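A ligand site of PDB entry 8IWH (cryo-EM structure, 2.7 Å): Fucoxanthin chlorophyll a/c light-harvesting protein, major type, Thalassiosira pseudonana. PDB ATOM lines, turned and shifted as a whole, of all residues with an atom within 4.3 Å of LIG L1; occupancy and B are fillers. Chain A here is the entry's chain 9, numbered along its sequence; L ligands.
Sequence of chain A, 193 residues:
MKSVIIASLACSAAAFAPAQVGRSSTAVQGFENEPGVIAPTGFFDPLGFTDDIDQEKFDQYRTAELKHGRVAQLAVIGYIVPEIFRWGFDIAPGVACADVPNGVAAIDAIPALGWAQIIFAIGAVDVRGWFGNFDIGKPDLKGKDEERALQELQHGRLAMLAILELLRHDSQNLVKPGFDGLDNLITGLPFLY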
ATOM      1  N   LYS A  67       5.222  -1.443 -17.929  1.00  0.00           N
ATOM      2  CA  LYS A  67       4.709  -1.719 -16.588  1.00  0.00           C
ATOM      3  C   LYS A  67       5.176  -3.075 -16.069  1.00  0.00           C
ATOM      4  O   LYS A  67       5.579  -3.188 -14.910  1.00  0.00           O
ATOM      5  CB  LYS A  67       3.181  -1.644 -16.580  1.00  0.00           C
ATOM      6  CG  LYS A  67       2.597  -1.375 -15.219  1.00  0.00           C
ATOM      7  CD  LYS A  67       1.145  -0.960 -15.295  1.00  0.00           C
ATOM      8  CE  LYS A  67       1.001   0.441 -15.835  1.00  0.00           C
ATOM      9  NZ  LYS A  67      -0.439   0.829 -15.939  1.00  0.00           N
ATOM     10  N   VAL A  71       7.528  -3.474 -12.684  1.00  0.00           N
ATOM     11  CA  VAL A  71       7.160  -4.304 -11.532  1.00  0.00           C
ATOM     12  C   VAL A  71       8.165  -5.422 -11.346  1.00  0.00           C
ATOM     13  O   VAL A  71       8.462  -5.810 -10.205  1.00  0.00           O
ATOM     14  CB  VAL A  71       5.717  -4.838 -11.663  1.00  0.00           C
ATOM     15  CG1 VAL A  71       4.744  -3.683 -11.859  1.00  0.00           C
ATOM     16  CG2 VAL A  71       5.587  -5.860 -12.778  1.00  0.00           C
ATOM     17  N   LEU A  74      11.118  -3.865  -9.458  1.00  0.00           N
ATOM     18  CA  LEU A  74      10.858  -3.716  -8.027  1.00  0.00           C
ATOM     19  C   LEU A  74      10.851  -5.073  -7.316  1.00  0.00           C
ATOM     20  O   LEU A  74      11.421  -5.199  -6.217  1.00  0.00           O
ATOM     21  CB  LEU A  74       9.534  -2.982  -7.808  1.00  0.00           C
ATOM     22  CG  LEU A  74       9.575  -1.479  -8.089  1.00  0.00           C
ATOM     23  CD1 LEU A  74       8.320  -0.817  -7.571  1.00  0.00           C
ATOM     24  CD2 LEU A  74      10.806  -0.838  -7.467  1.00  0.00           C
ATOM     25  N   PHE A  89       6.878  -3.798  11.823  1.00  0.00           N
ATOM     26  CA  PHE A  89       5.440  -3.792  11.571  1.00  0.00           C
ATOM     27  C   PHE A  89       4.779  -5.009  12.199  1.00  0.00           C
ATOM     28  O   PHE A  89       5.439  -5.981  12.608  1.00  0.00           O
ATOM     29  CB  PHE A  89       5.155  -3.773  10.071  1.00  0.00           C
ATOM     30  CG  PHE A  89       5.258  -2.414   9.449  1.00  0.00           C
ATOM     31  CD1 PHE A  89       5.319  -1.282  10.246  1.00  0.00           C
ATOM     32  CD2 PHE A  89       5.276  -2.271   8.076  1.00  0.00           C
ATOM     33  CE1 PHE A  89       5.402  -0.030   9.662  1.00  0.00           C
ATOM     34  CE2 PHE A  89       5.368  -1.022   7.502  1.00  0.00           C
ATOM     35  CZ  PHE A  89       5.426   0.100   8.290  1.00  0.00           C
ATOM     36  N   ASP A  90       3.461  -4.959  12.272  1.00  0.00           N
ATOM     37  CA  ASP A  90       2.667  -6.073  12.776  1.00  0.00           C
ATOM     38  C   ASP A  90       1.736  -6.661  11.725  1.00  0.00           C
ATOM     39  O   ASP A  90       1.634  -7.889  11.636  1.00  0.00           O
ATOM     40  CB  ASP A  90       1.837  -5.615  13.985  1.00  0.00           C
ATOM     41  N   ILE A  91       1.072  -5.826  10.918  1.00  0.00           N
ATOM     42  CA  ILE A  91       0.118  -6.274   9.908  1.00  0.00           C
ATOM     43  C   ILE A  91      -0.892  -7.206  10.544  1.00  0.00           C
ATOM     44  O   ILE A  91      -1.003  -8.378  10.174  1.00  0.00           O
ATOM     45  CB  ILE A  91       0.831  -6.940   8.721  1.00  0.00           C
ATOM     46  CG1 ILE A  91       2.121  -6.203   8.380  1.00  0.00           C
ATOM     47  CG2 ILE A  91      -0.075  -6.974   7.504  1.00  0.00           C
ATOM     48  CD1 ILE A  91       2.888  -6.825   7.244  1.00  0.00           C
ATOM     49  N   ALA A  92      -1.654  -6.694  11.518  1.00  0.00           N
ATOM     50  CA  ALA A  92      -2.564  -7.540  12.282  1.00  0.00           C
ATOM     51  C   ALA A  92      -1.773  -8.275  13.351  1.00  0.00           C
ATOM     52  O   ALA A  92      -0.596  -7.981  13.573  1.00  0.00           O
ATOM     53  N   ILE A 118      -4.126  -3.721   0.398  1.00  0.00           N
ATOM     54  CA  ILE A 118      -2.912  -3.332  -0.312  1.00  0.00           C
ATOM     55  C   ILE A 118      -3.149  -3.291  -1.811  1.00  0.00           C
ATOM     56  O   ILE A 118      -2.724  -2.358  -2.505  1.00  0.00           O
ATOM     57  CB  ILE A 118      -1.755  -4.291   0.053  1.00  0.00           C
ATOM     58  CG1 ILE A 118      -1.444  -4.213   1.546  1.00  0.00           C
ATOM     59  CG2 ILE A 118      -0.513  -3.958  -0.757  1.00  0.00           C
ATOM     60  CD1 ILE A 118      -0.278  -5.086   1.966  1.00  0.00           C
ATOM     61  N   ILE A 122      -2.816  -0.005  -4.294  1.00  0.00           N
ATOM     62  CA  ILE A 122      -1.955  -0.025  -5.459  1.00  0.00           C
ATOM     63  C   ILE A 122      -2.761   0.271  -6.715  1.00  0.00           C
ATOM     64  O   ILE A 122      -2.311   0.984  -7.612  1.00  0.00           O
ATOM     65  CB  ILE A 122      -1.213  -1.369  -5.573  1.00  0.00           C
ATOM     66  CG1 ILE A 122      -0.308  -1.592  -4.369  1.00  0.00           C
ATOM     67  CG2 ILE A 122      -0.391  -1.422  -6.850  1.00  0.00           C
ATOM     68  CD1 ILE A 122       0.149  -3.017  -4.223  1.00  0.00           C
ATOM     69  N   VAL A 125      -3.564   3.953  -7.066  1.00  0.00           N
ATOM     70  CA  VAL A 125      -2.391   4.620  -7.641  1.00  0.00           C
ATOM     71  C   VAL A 125      -2.291   4.317  -9.134  1.00  0.00           C
ATOM     72  O   VAL A 125      -1.937   5.187  -9.938  1.00  0.00           O
ATOM     73  CB  VAL A 125      -1.117   4.224  -6.884  1.00  0.00           C
ATOM     74  CG1 VAL A 125       0.087   4.944  -7.454  1.00  0.00           C
ATOM     75  CG2 VAL A 125      -1.266   4.519  -5.407  1.00  0.00           C
ATOM     76  N   ASP A 126      -2.598   3.084  -9.526  1.00  0.00           N
ATOM     77  CA  ASP A 126      -2.415   2.647 -10.907  1.00  0.00           C
ATOM     78  C   ASP A 126      -3.361   3.375 -11.855  1.00  0.00           C
ATOM     79  O   ASP A 126      -2.935   3.865 -12.909  1.00  0.00           O
ATOM     80  CB  ASP A 126      -2.626   1.129 -10.985  1.00  0.00           C
ATOM     81  CG  ASP A 126      -2.267   0.555 -12.350  1.00  0.00           C
ATOM     82  OD1 ASP A 126      -1.644   1.260 -13.163  1.00  0.00           O
ATOM     83  OD2 ASP A 126      -2.623  -0.621 -12.612  1.00  0.00           O
HETATM   84  C1  LIG L   1       1.526  -0.014   2.892  1.00  0.00           C
HETATM   85  O1  LIG L   1       5.044  -1.499  -9.300  1.00  0.00           O
HETATM   86  C2  LIG L   1       1.806  -1.475   2.994  1.00  0.00           C
HETATM   87  C3  LIG L   1       3.605  -1.110  -6.133  1.00  0.00           C
HETATM   88  C4  LIG L   1       4.213  -1.741  -7.135  1.00  0.00           C
HETATM   89  C5  LIG L   1       4.625  -3.172  -7.018  1.00  0.00           C
HETATM   90  C6  LIG L   1       4.472  -0.996  -8.357  1.00  0.00           C
HETATM   91  C7  LIG L   1       3.993   0.432  -8.413  1.00  0.00           C
HETATM   92  C8  LIG L   1       3.211   0.715  -9.685  1.00  0.00           C
HETATM   93  C9  LIG L   1       1.753   0.270  -9.896  1.00  0.00           C
HETATM   94  C10 LIG L   1       1.292   0.439 -11.329  1.00  0.00           C
HETATM   95  C11 LIG L   1       1.823   1.740 -11.902  1.00  0.00           C
HETATM   96  C12 LIG L   1       3.297   1.507 -12.169  1.00  0.00           C
HETATM   97  C13 LIG L   1       2.346  -2.146   1.976  1.00  0.00           C
HETATM   98  C14 LIG L   1       4.005   1.334 -10.838  1.00  0.00           C
HETATM   99  C15 LIG L   1       5.470   1.736 -10.851  1.00  0.00           C
HETATM  100  C16 LIG L   1       0.865   1.124  -8.995  1.00  0.00           C
HETATM  101  C17 LIG L   1       1.569  -1.191  -9.530  1.00  0.00           C
HETATM  102  C18 LIG L   1       1.474  -2.198   4.232  1.00  0.00           C
HETATM  103  C19 LIG L   1       0.867  -1.574   5.241  1.00  0.00           C
HETATM  104  C20 LIG L   1       0.560  -2.375   6.413  1.00  0.00           C
HETATM  105  C21 LIG L   1      -0.211  -1.905   7.403  1.00  0.00           C
HETATM  106  C22 LIG L   1      -0.784  -0.520   7.344  1.00  0.00           C
HETATM  107  C23 LIG L   1      -0.470  -2.787   8.548  1.00  0.00           C
HETATM  108  C24 LIG L   1       2.673  -1.457   0.734  1.00  0.00           C
HETATM  109  C25 LIG L   1      -0.835  -2.350   9.655  1.00  0.00           C
HETATM  110  C26 LIG L   1      -1.194  -1.940  10.778  1.00  0.00           C
HETATM  111  C27 LIG L   1      -2.640  -1.625  11.023  1.00  0.00           C
HETATM  112  C28 LIG L   1      -2.866  -1.372  12.510  1.00  0.00           C
HETATM  113  C29 LIG L   1      -1.878  -0.426  13.176  1.00  0.00           C
HETATM  114  C30 LIG L   1      -0.450  -0.505  12.630  1.00  0.00           C
HETATM  115  C31 LIG L   1      -0.171  -1.798  11.876  1.00  0.00           C
HETATM  116  C32 LIG L   1       1.232  -1.774  11.294  1.00  0.00           C
HETATM  117  C33 LIG L   1      -3.327   1.194  14.100  1.00  0.00           C
HETATM  118  C34 LIG L   1      -4.632   1.843  13.717  1.00  0.00           C
HETATM  119  C35 LIG L   1       2.463  -2.104  -0.400  1.00  0.00           C
HETATM  120  C36 LIG L   1      -3.445  -2.838  10.595  1.00  0.00           C
HETATM  121  C37 LIG L   1      -3.056  -0.415  10.190  1.00  0.00           C
HETATM  122  C38 LIG L   1       2.756  -1.480  -1.687  1.00  0.00           C
HETATM  123  C39 LIG L   1       3.680  -2.023  -2.486  1.00  0.00           C
HETATM  124  C40 LIG L   1       4.421  -3.253  -2.057  1.00  0.00           C
HETATM  125  C41 LIG L   1       3.967  -1.380  -3.781  1.00  0.00           C
HETATM  126  C42 LIG L   1       3.316  -1.772  -4.870  1.00  0.00           C
HETATM  127  O2  LIG L   1       3.304   2.122  -9.883  1.00  0.00           O
HETATM  128  O3  LIG L   1       1.129   2.060 -13.107  1.00  0.00           O
HETATM  129  O4  LIG L   1      -0.286  -2.912  12.765  1.00  0.00           O
HETATM  130  O5  LIG L   1      -2.352   0.908  13.069  1.00  0.00           O
HETATM  131  O6  LIG L   1      -3.062   0.893  15.245  1.00  0.00           O
HETATM  132 MG1  LG2 L   2      -6.565  -1.357   7.326  1.00  0.00          MG
HETATM  133  C1  LG2 L   2      -6.208  -4.586   8.529  1.00  0.00           C
HETATM  134  C2  LG2 L   2      -9.382  -0.967   9.183  1.00  0.00           C
HETATM  135  C3  LG2 L   2      -6.818   1.868   6.163  1.00  0.00           C
HETATM  136  C4  LG2 L   2      -3.631  -1.808   5.383  1.00  0.00           C
HETATM  137  N1  LG2 L   2      -7.611  -2.603   8.626  1.00  0.00           N
HETATM  138  C5  LG2 L   2      -7.303  -3.916   9.009  1.00  0.00           C
HETATM  139  C6  LG2 L   2      -8.353  -4.470   9.974  1.00  0.00           C
HETATM  140  C7  LG2 L   2      -9.368  -3.311  10.122  1.00  0.00           C
HETATM  141  C8  LG2 L   2      -8.765  -2.207   9.252  1.00  0.00           C
HETATM  142  C9  LG2 L   2     -10.736  -3.701   9.647  1.00  0.00           C
HETATM  143  C10 LG2 L   2      -7.798  -4.897  11.327  1.00  0.00           C
HETATM  144  C11 LG2 L   2      -6.740  -3.951  11.859  1.00  0.00           C
HETATM  145  C12 LG2 L   2      -5.999  -4.637  12.969  1.00  0.00           C
HETATM  146  O1  LG2 L   2      -6.445  -5.340  13.875  1.00  0.00           O
HETATM  147  O2  LG2 L   2      -4.645  -4.429  12.905  1.00  0.00           O
HETATM  148  N2  LG2 L   2      -7.871   0.153   7.595  1.00  0.00           N
HETATM  149  C13 LG2 L   2      -8.934   0.129   8.434  1.00  0.00           C
HETATM  150  C14 LG2 L   2      -9.591   1.466   8.448  1.00  0.00           C
HETATM  151  C15 LG2 L   2      -8.876   2.272   7.598  1.00  0.00           C
HETATM  152  C16 LG2 L   2      -7.761   1.443   7.045  1.00  0.00           C
HETATM  153  C17 LG2 L   2     -10.781   1.756   9.255  1.00  0.00           C
HETATM  154  C18 LG2 L   2      -9.060   3.651   7.236  1.00  0.00           C
HETATM  155  C19 LG2 L   2      -9.280   4.643   8.098  1.00  0.00           C
HETATM  156  N3  LG2 L   2      -5.434  -0.198   6.002  1.00  0.00           N
HETATM  157  C20 LG2 L   2      -5.727   1.102   5.660  1.00  0.00           C
HETATM  158  C21 LG2 L   2      -4.737   1.598   4.716  1.00  0.00           C
HETATM  159  C22 LG2 L   2      -3.832   0.572   4.499  1.00  0.00           C
HETATM  160  C23 LG2 L   2      -4.275  -0.557   5.313  1.00  0.00           C
HETATM  161  C24 LG2 L   2      -4.737   2.945   4.135  1.00  0.00           C
HETATM  162  N4  LG2 L   2      -5.194  -2.802   6.985  1.00  0.00           N
HETATM  163  C25 LG2 L   2      -4.046  -2.871   6.160  1.00  0.00           C
HETATM  164  C26 LG2 L   2      -3.424  -4.198   6.299  1.00  0.00           C
HETATM  165  C27 LG2 L   2      -4.196  -4.885   7.215  1.00  0.00           C
HETATM  166  C28 LG2 L   2      -5.297  -3.984   7.598  1.00  0.00           C
HETATM  167  C29 LG2 L   2      -2.209  -4.625   5.608  1.00  0.00           C
HETATM  168  C30 LG2 L   2      -4.385  -6.130   7.929  1.00  0.00           C
HETATM  169  O3  LG2 L   2      -3.698  -7.149   7.926  1.00  0.00           O
HETATM  170  C31 LG2 L   2      -5.677  -5.977   8.783  1.00  0.00           C
HETATM  171  C32 LG2 L   2      -6.700  -7.028   8.425  1.00  0.00           C
HETATM  172  O4  LG2 L   2      -7.001  -7.419   7.298  1.00  0.00           O
HETATM  173  O5  LG2 L   2      -7.351  -7.564   9.488  1.00  0.00           O
HETATM  174  C33 LG2 L   2      -7.148  -8.957   9.750  1.00  0.00           C
HETATM  175 MG1  LG3 L   3       8.572  -5.968   0.194  1.00  0.00          MG
HETATM  176  C1  LG3 L   3       8.168  -7.118   3.442  1.00  0.00           C
HETATM  177  C2  LG3 L   3       5.626  -7.431  -0.682  1.00  0.00           C
HETATM  178  C3  LG3 L   3       8.936  -4.682  -2.960  1.00  0.00           C
HETATM  179  C4  LG3 L   3      11.622  -4.451   1.165  1.00  0.00           C
HETATM  180  N1  LG3 L   3       7.155  -7.097   1.230  1.00  0.00           N
HETATM  181  C5  LG3 L   3       7.155  -7.458   2.584  1.00  0.00           C
HETATM  182  C6  LG3 L   3       5.914  -8.280   2.934  1.00  0.00           C
HETATM  183  C7  LG3 L   3       5.197  -8.456   1.572  1.00  0.00           C
HETATM  184  C8  LG3 L   3       6.028  -7.604   0.628  1.00  0.00           C
HETATM  185  C9  LG3 L   3       5.154  -9.898   1.144  1.00  0.00           C
HETATM  186  C10 LG3 L   3       4.988  -7.577   3.915  1.00  0.00           C
HETATM  187  C11 LG3 L   3       5.196  -6.074   4.021  1.00  0.00           C
HETATM  188  C12 LG3 L   3       4.518  -5.345   2.905  1.00  0.00           C
HETATM  189  O1  LG3 L   3       3.321  -5.049   2.796  1.00  0.00           O
HETATM  190  O2  LG3 L   3       5.376  -4.974   1.910  1.00  0.00           O
HETATM  191  N2  LG3 L   3       7.506  -6.068  -1.502  1.00  0.00           N
HETATM  192  C13 LG3 L   3       6.305  -6.680  -1.652  1.00  0.00           C
HETATM  193  C14 LG3 L   3       5.779  -6.444  -3.026  1.00  0.00           C
HETATM  194  C15 LG3 L   3       6.715  -5.664  -3.675  1.00  0.00           C
HETATM  195  C16 LG3 L   3       7.819  -5.416  -2.721  1.00  0.00           C
HETATM  196  C17 LG3 L   3       4.504  -6.993  -3.484  1.00  0.00           C
HETATM  197  C18 LG3 L   3       6.734  -5.137  -5.011  1.00  0.00           C
HETATM  198  C19 LG3 L   3       6.259  -5.746  -6.107  1.00  0.00           C
HETATM  199  N3  LG3 L   3      10.036  -4.802  -0.728  1.00  0.00           N
HETATM  200  C20 LG3 L   3       9.973  -4.396  -2.032  1.00  0.00           C
HETATM  201  C21 LG3 L   3      11.154  -3.591  -2.350  1.00  0.00           C
HETATM  202  C22 LG3 L   3      11.911  -3.526  -1.185  1.00  0.00           C
HETATM  203  C23 LG3 L   3      11.193  -4.283  -0.161  1.00  0.00           C
HETATM  204  C24 LG3 L   3      11.437  -3.005  -3.658  1.00  0.00           C
HETATM  205  C25 LG3 L   3      13.183  -2.811  -1.013  1.00  0.00           C
HETATM  206  C26 LG3 L   3      13.007  -1.383  -0.572  1.00  0.00           C
HETATM  207  N4  LG3 L   3       9.694  -5.803   1.875  1.00  0.00           N
HETATM  208  C27 LG3 L   3      10.933  -5.159   2.136  1.00  0.00           C
HETATM  209  C28 LG3 L   3      11.297  -5.381   3.556  1.00  0.00           C
HETATM  210  C29 LG3 L   3      10.275  -6.122   4.099  1.00  0.00           C
HETATM  211  C30 LG3 L   3       9.302  -6.357   3.017  1.00  0.00           C
HETATM  212  C31 LG3 L   3      12.506  -4.873   4.191  1.00  0.00           C
HETATM  213  C32 LG3 L   3       9.758  -6.768   5.292  1.00  0.00           C
HETATM  214  O3  LG3 L   3      10.229  -6.805   6.419  1.00  0.00           O
HETATM  215  C33 LG3 L   3       8.397  -7.430   4.903  1.00  0.00           C
HETATM  216  C34 LG3 L   3       8.398  -8.907   5.161  1.00  0.00           C
HETATM  217  O4  LG3 L   3       9.026  -9.781   4.564  1.00  0.00           O
HETATM  218  O5  LG3 L   3       7.582  -9.288   6.183  1.00  0.00           O
HETATM  219  C35 LG3 L   3       8.009 -10.411   6.961  1.00  0.00           C
HETATM  220  C36 LG3 L   3       6.321  -3.925   2.191  1.00  0.00           C
HETATM  221  C37 LG3 L   3       5.977  -2.795   1.300  1.00  0.00           C
HETATM  222  C38 LG3 L   3       6.884  -2.086   0.599  1.00  0.00           C
HETATM  223  C39 LG3 L   3       8.327  -2.374   0.659  1.00  0.00           C
HETATM  224  C40 LG3 L   3       6.468  -0.963  -0.279  1.00  0.00           C
HETATM  225  C41 LG3 L   3       7.289  -0.869  -1.552  1.00  0.00           C
HETATM  226  C42 LG3 L   3       6.573  -0.027  -2.582  1.00  0.00           C
HETATM  227  C43 LG3 L   3       7.542   0.753  -3.459  1.00  0.00           C
HETATM  228  C44 LG3 L   3       8.561   1.470  -2.600  1.00  0.00           C
HETATM  229  C45 LG3 L   3       6.792   1.763  -4.324  1.00  0.00           C
HETATM  230 MG1  LG4 L   4       4.285   7.623  -4.382  1.00  0.00          MG
HETATM  231  C1  LG4 L   4       6.308   9.353  -6.608  1.00  0.00           C
HETATM  232  C2  LG4 L   4       3.956   5.104  -6.633  1.00  0.00           C
HETATM  233  C3  LG4 L   4       2.382   5.905  -2.087  1.00  0.00           C
HETATM  234  C4  LG4 L   4       4.678  10.262  -2.049  1.00  0.00           C
HETATM  235  N1  LG4 L   4       5.005   7.316  -6.312  1.00  0.00           N
HETATM  236  C5  LG4 L   4       5.849   8.148  -7.068  1.00  0.00           C
HETATM  237  C6  LG4 L   4       6.144   7.538  -8.434  1.00  0.00           C
HETATM  238  C7  LG4 L   4       5.290   6.245  -8.445  1.00  0.00           C
HETATM  239  C8  LG4 L   4       4.700   6.195  -7.029  1.00  0.00           C
HETATM  240  C9  LG4 L   4       4.209   6.282  -9.488  1.00  0.00           C
HETATM  241  C10 LG4 L   4       7.622   7.198  -8.567  1.00  0.00           C
HETATM  242  N2  LG4 L   4       3.338   5.846  -4.362  1.00  0.00           N
HETATM  243  C11 LG4 L   4       3.349   4.942  -5.380  1.00  0.00           C
HETATM  244  C12 LG4 L   4       2.600   3.726  -4.965  1.00  0.00           C
HETATM  245  C13 LG4 L   4       2.157   3.929  -3.684  1.00  0.00           C
HETATM  246  C14 LG4 L   4       2.607   5.297  -3.289  1.00  0.00           C
HETATM  247  C15 LG4 L   4       2.429   2.555  -5.829  1.00  0.00           C
HETATM  248  C16 LG4 L   4       1.375   3.069  -2.836  1.00  0.00           C
HETATM  249  C17 LG4 L   4       1.781   2.593  -1.653  1.00  0.00           C
HETATM  250  N3  LG4 L   4       3.631   8.023  -2.439  1.00  0.00           N
HETATM  251  C18 LG4 L   4       2.859   7.192  -1.690  1.00  0.00           C
HETATM  252  C19 LG4 L   4       2.591   7.788  -0.383  1.00  0.00           C
HETATM  253  C20 LG4 L   4       3.246   9.006  -0.366  1.00  0.00           C
HETATM  254  C21 LG4 L   4       3.899   9.155  -1.666  1.00  0.00           C
HETATM  255  C22 LG4 L   4       1.797   7.162   0.679  1.00  0.00           C
HETATM  256  C23 LG4 L   4       3.287   9.986   0.732  1.00  0.00           C
HETATM  257  C24 LG4 L   4       4.587   9.937   1.502  1.00  0.00           C
HETATM  258  N4  LG4 L   4       5.208   9.419  -4.296  1.00  0.00           N
HETATM  259  C25 LG4 L   4       5.311  10.399  -3.274  1.00  0.00           C
HETATM  260  C26 LG4 L   4       6.156  11.507  -3.749  1.00  0.00           C
HETATM  261  C27 LG4 L   4       6.559  11.162  -5.023  1.00  0.00           C
HETATM  262  C28 LG4 L   4       5.952   9.847  -5.307  1.00  0.00           C
HETATM  263  C29 LG4 L   4       6.471  12.707  -2.971  1.00  0.00           C
HETATM  264  C30 LG4 L   4       7.319  11.554  -6.196  1.00  0.00           C
HETATM  265  O1  LG4 L   4       7.955  12.585  -6.400  1.00  0.00           O
HETATM  266  C31 LG4 L   4       7.213  10.394  -7.225  1.00  0.00           C
HETATM  267  C32 LG4 L   4       6.703  10.859  -8.561  1.00  0.00           C
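Merely in contact with LIG L1: Ile 122 (3.3 Å), Val 71 (3.4 Å), Ile 118 (3.5 Å), Asp 90 (3.6 Å), Ile 91 (3.7 Å) and Leu 74 (3.8 Å).
Of the 11 residues printed, 8 come within 4 Å of LIG L1.
Along chain A the residues within 4 Å of LIG L1 span positions 67 to 126.
The side-chain carboxylate of Asp 126 is in salt-bridge range of the side-chain amino group of Lys 67.
OD1 of Asp 126 sits at hydrogen-bond distance from O3 of LIG L1 (2.9 Å).
An oxygen (O3) of LIG L1 sits close to the side-chain amino group (NZ) of Lys 67 (3.5 Å).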
